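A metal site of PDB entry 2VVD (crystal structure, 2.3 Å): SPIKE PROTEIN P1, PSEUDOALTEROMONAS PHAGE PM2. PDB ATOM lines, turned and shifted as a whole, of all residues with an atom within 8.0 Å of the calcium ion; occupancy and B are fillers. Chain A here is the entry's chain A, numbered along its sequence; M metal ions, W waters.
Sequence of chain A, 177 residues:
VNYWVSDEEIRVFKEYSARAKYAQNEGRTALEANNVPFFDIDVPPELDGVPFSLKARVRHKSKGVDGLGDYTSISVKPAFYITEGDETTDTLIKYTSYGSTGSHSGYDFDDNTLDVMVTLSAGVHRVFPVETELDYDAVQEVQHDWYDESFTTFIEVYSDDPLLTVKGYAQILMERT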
ATOM      1  N   THR A  72     -14.123 -31.553   0.387  1.00  0.00           N
ATOM      2  CA  THR A  72     -14.786 -30.316   0.740  1.00  0.00           C
ATOM      3  C   THR A  72     -15.965 -30.078  -0.214  1.00  0.00           C
ATOM      4  O   THR A  72     -15.805 -30.161  -1.439  1.00  0.00           O
ATOM      5  CB  THR A  72     -13.796 -29.128   0.688  1.00  0.00           C
ATOM      6  OG1 THR A  72     -12.760 -29.357   1.664  1.00  0.00           O
ATOM      7  CG2 THR A  72     -14.490 -27.810   0.991  1.00  0.00           C
ATOM      8  N   SER A  73     -17.142 -29.814   0.346  1.00  0.00           N
ATOM      9  CA  SER A  73     -18.326 -29.547  -0.447  1.00  0.00           C
ATOM     10  C   SER A  73     -18.314 -28.108  -0.949  1.00  0.00           C
ATOM     11  O   SER A  73     -18.109 -27.179  -0.157  1.00  0.00           O
ATOM     12  CB  SER A  73     -19.594 -29.778   0.382  1.00  0.00           C
ATOM     13  OG  SER A  73     -20.749 -29.411  -0.369  1.00  0.00           O
ATOM     14  N   ILE A  74     -18.515 -27.920  -2.254  1.00  0.00           N
ATOM     15  CA  ILE A  74     -18.509 -26.595  -2.874  1.00  0.00           C
ATOM     16  C   ILE A  74     -19.802 -26.317  -3.630  1.00  0.00           C
ATOM     17  O   ILE A  74     -20.093 -26.957  -4.648  1.00  0.00           O
ATOM     18  CB  ILE A  74     -17.306 -26.420  -3.829  1.00  0.00           C
ATOM     19  CG1 ILE A  74     -15.993 -26.387  -3.045  1.00  0.00           C
ATOM     20  CG2 ILE A  74     -17.464 -25.162  -4.689  1.00  0.00           C
ATOM     21  CD1 ILE A  74     -15.872 -25.225  -2.050  1.00  0.00           C
ATOM     22  N   SER A  75     -20.582 -25.370  -3.120  1.00  0.00           N
ATOM     23  CA  SER A  75     -21.838 -24.957  -3.743  1.00  0.00           C
ATOM     24  C   SER A  75     -21.511 -24.018  -4.907  1.00  0.00           C
ATOM     25  O   SER A  75     -20.666 -23.123  -4.772  1.00  0.00           O
ATOM     26  CB  SER A  75     -22.735 -24.230  -2.737  1.00  0.00           C
ATOM     27  OG  SER A  75     -23.164 -25.099  -1.696  1.00  0.00           O
ATOM     28  N   VAL A  76     -22.202 -24.236  -6.037  1.00  0.00           N
ATOM     29  CA  VAL A  76     -21.983 -23.451  -7.264  1.00  0.00           C
ATOM     30  C   VAL A  76     -23.302 -23.012  -7.904  1.00  0.00           C
ATOM     31  O   VAL A  76     -24.335 -23.674  -7.791  1.00  0.00           O
ATOM     32  CB  VAL A  76     -21.147 -24.220  -8.313  1.00  0.00           C
ATOM     33  CG1 VAL A  76     -19.748 -24.486  -7.795  1.00  0.00           C
ATOM     34  CG2 VAL A  76     -21.844 -25.520  -8.711  1.00  0.00           C
ATOM     35  N   THR A 101     -23.859 -28.833  -5.714  1.00  0.00           N
ATOM     36  CA  THR A 101     -23.125 -28.851  -4.449  1.00  0.00           C
ATOM     37  C   THR A 101     -22.264 -30.105  -4.309  1.00  0.00           C
ATOM     38  O   THR A 101     -22.198 -30.927  -5.219  1.00  0.00           O
ATOM     39  CB  THR A 101     -24.080 -28.692  -3.246  1.00  0.00           C
ATOM     40  OG1 THR A 101     -23.332 -28.463  -2.046  1.00  0.00           O
ATOM     41  CG2 THR A 101     -24.961 -29.930  -3.075  1.00  0.00           C
ATOM     42  N   GLY A 102     -21.570 -30.227  -3.175  1.00  0.00           N
ATOM     43  CA  GLY A 102     -20.661 -31.344  -2.921  1.00  0.00           C
ATOM     44  C   GLY A 102     -19.283 -31.177  -3.560  1.00  0.00           C
ATOM     45  O   GLY A 102     -18.943 -30.098  -4.046  1.00  0.00           O
ATOM     46  N   GLU A 133     -21.811 -17.928  -6.726  1.00  0.00           N
ATOM     47  CA  GLU A 133     -21.775 -18.463  -5.365  1.00  0.00           C
ATOM     48  C   GLU A 133     -20.342 -18.545  -4.855  1.00  0.00           C
ATOM     49  O   GLU A 133     -19.513 -19.244  -5.431  1.00  0.00           O
ATOM     50  CB  GLU A 133     -22.440 -19.848  -5.329  1.00  0.00           C
ATOM     51  CG  GLU A 133     -22.619 -20.451  -3.921  1.00  0.00           C
ATOM     52  CD  GLU A 133     -23.789 -19.850  -3.132  1.00  0.00           C
ATOM     53  OE1 GLU A 133     -24.383 -18.859  -3.586  1.00  0.00           O
ATOM     54  OE2 GLU A 133     -24.103 -20.382  -2.042  1.00  0.00           O
ATOM     55  N   LEU A 134     -20.061 -17.809  -3.781  1.00  0.00           N
ATOM     56  CA  LEU A 134     -18.781 -17.883  -3.084  1.00  0.00           C
ATOM     57  C   LEU A 134     -18.939 -18.822  -1.901  1.00  0.00           C
ATOM     58  O   LEU A 134     -19.599 -18.488  -0.915  1.00  0.00           O
ATOM     59  CB  LEU A 134     -18.336 -16.485  -2.614  1.00  0.00           C
ATOM     60  CG  LEU A 134     -17.041 -16.394  -1.793  1.00  0.00           C
ATOM     61  CD1 LEU A 134     -15.826 -16.800  -2.609  1.00  0.00           C
ATOM     62  CD2 LEU A 134     -16.852 -14.990  -1.236  1.00  0.00           C
ATOM     63  N   ASP A 135     -18.347 -20.000  -1.989  1.00  0.00           N
ATOM     64  CA  ASP A 135     -18.550 -21.032  -0.981  1.00  0.00           C
ATOM     65  C   ASP A 135     -17.730 -20.731   0.268  1.00  0.00           C
ATOM     66  O   ASP A 135     -16.545 -20.421   0.180  1.00  0.00           O
ATOM     67  CB  ASP A 135     -18.198 -22.408  -1.537  1.00  0.00           C
ATOM     68  CG  ASP A 135     -18.671 -23.522  -0.639  1.00  0.00           C
ATOM     69  OD1 ASP A 135     -19.772 -24.056  -0.899  1.00  0.00           O
ATOM     70  OD2 ASP A 135     -17.966 -23.865   0.328  1.00  0.00           O
ATOM     71  N   TYR A 136     -18.371 -20.838   1.427  1.00  0.00           N
ATOM     72  CA  TYR A 136     -17.738 -20.481   2.693  1.00  0.00           C
ATOM     73  C   TYR A 136     -16.526 -21.371   3.025  1.00  0.00           C
ATOM     74  O   TYR A 136     -15.558 -20.887   3.601  1.00  0.00           O
ATOM     75  CB  TYR A 136     -18.767 -20.534   3.822  1.00  0.00           C
ATOM     76  CG  TYR A 136     -18.239 -20.027   5.137  1.00  0.00           C
ATOM     77  CD1 TYR A 136     -17.988 -18.665   5.328  1.00  0.00           C
ATOM     78  CD2 TYR A 136     -17.992 -20.900   6.196  1.00  0.00           C
ATOM     79  CE1 TYR A 136     -17.511 -18.186   6.544  1.00  0.00           C
ATOM     80  CE2 TYR A 136     -17.515 -20.430   7.412  1.00  0.00           C
ATOM     81  CZ  TYR A 136     -17.273 -19.088   7.584  1.00  0.00           C
ATOM     82  OH  TYR A 136     -16.800 -18.628   8.791  1.00  0.00           O
ATOM     83  N   ASP A 137     -16.579 -22.647   2.656  1.00  0.00           N
ATOM     84  CA  ASP A 137     -15.413 -23.540   2.827  1.00  0.00           C
ATOM     85  C   ASP A 137     -14.216 -23.054   2.025  1.00  0.00           C
ATOM     86  O   ASP A 137     -13.084 -23.123   2.483  1.00  0.00           O
ATOM     87  CB  ASP A 137     -15.751 -24.976   2.440  1.00  0.00           C
ATOM     88  CG  ASP A 137     -16.867 -25.579   3.270  1.00  0.00           C
ATOM     89  OD1 ASP A 137     -16.864 -25.406   4.521  1.00  0.00           O
ATOM     90  OD2 ASP A 137     -17.751 -26.227   2.684  1.00  0.00           O
ATOM     91  N   ALA A 138     -14.475 -22.564   0.811  1.00  0.00           N
ATOM     92  CA  ALA A 138     -13.441 -21.966  -0.037  1.00  0.00           C
ATOM     93  C   ALA A 138     -12.887 -20.692   0.612  1.00  0.00           C
ATOM     94  O   ALA A 138     -11.675 -20.455   0.589  1.00  0.00           O
ATOM     95  CB  ALA A 138     -14.004 -21.648  -1.411  1.00  0.00           C
ATOM     96  N   GLU A 141     -10.750 -22.126   3.623  1.00  0.00           N
ATOM     97  CA  GLU A 141      -9.607 -22.979   3.293  1.00  0.00           C
ATOM     98  C   GLU A 141      -8.564 -22.270   2.442  1.00  0.00           C
ATOM     99  O   GLU A 141      -7.374 -22.326   2.753  1.00  0.00           O
ATOM    100  CB  GLU A 141     -10.058 -24.251   2.564  1.00  0.00           C
ATOM    101  CG  GLU A 141     -10.699 -25.296   3.455  1.00  0.00           C
ATOM    102  CD  GLU A 141     -10.949 -26.603   2.712  1.00  0.00           C
ATOM    103  OE1 GLU A 141     -10.137 -26.974   1.841  1.00  0.00           O
ATOM    104  OE2 GLU A 141     -11.962 -27.276   3.016  1.00  0.00           O
HETATM  105 CA    CA M   1     -19.469 -25.686   1.097  1.00  0.00          CA
HETATM  106  O   HOH W   1     -21.361 -26.699   0.058  1.00  0.00           O
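OG of Ser 73 is in hydrogen-bond range of OG1 of Thr 101, 3.2 Å away.
The side-chain carboxylate (OD1) of Asp 135 sits close to the backbone NH (N) of Ser 75 (2.7 Å).
The backbone NH of Gly 102 is in hydrogen-bond range of the side-chain hydroxyl of Ser 73 (3.0 Å).
Of the 14 residues printed, 3 come within 4 Å of the calcium ion.
Along chain A the residues within 4 Å of the calcium ion span positions 73 to 137.
The nearest printed residue that does not touch the calcium ion is Ile 74 (4.1 Å).
The backbone carbonyl oxygen (O) of Ser 73 is bound to the calcium ion (2.4 Å).
Water W1 is bound to the calcium ion, 2.4 Å away.
The calcium ion is bound by OD2 of Asp 137, at 2.4 Å.
The side-chain carboxylate (OD2) of Asp 135 binds the calcium ion, at 2.5 Å.
The calcium ion is bound by OD1 of Asp 135 (2.6 Å).
Water W1 lies within hydrogen-bond range of OG of Ser 73 (2.8 Å), OG of Ser 75 (3.0 Å) and OG1 of Thr 101 (3.4 Å).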
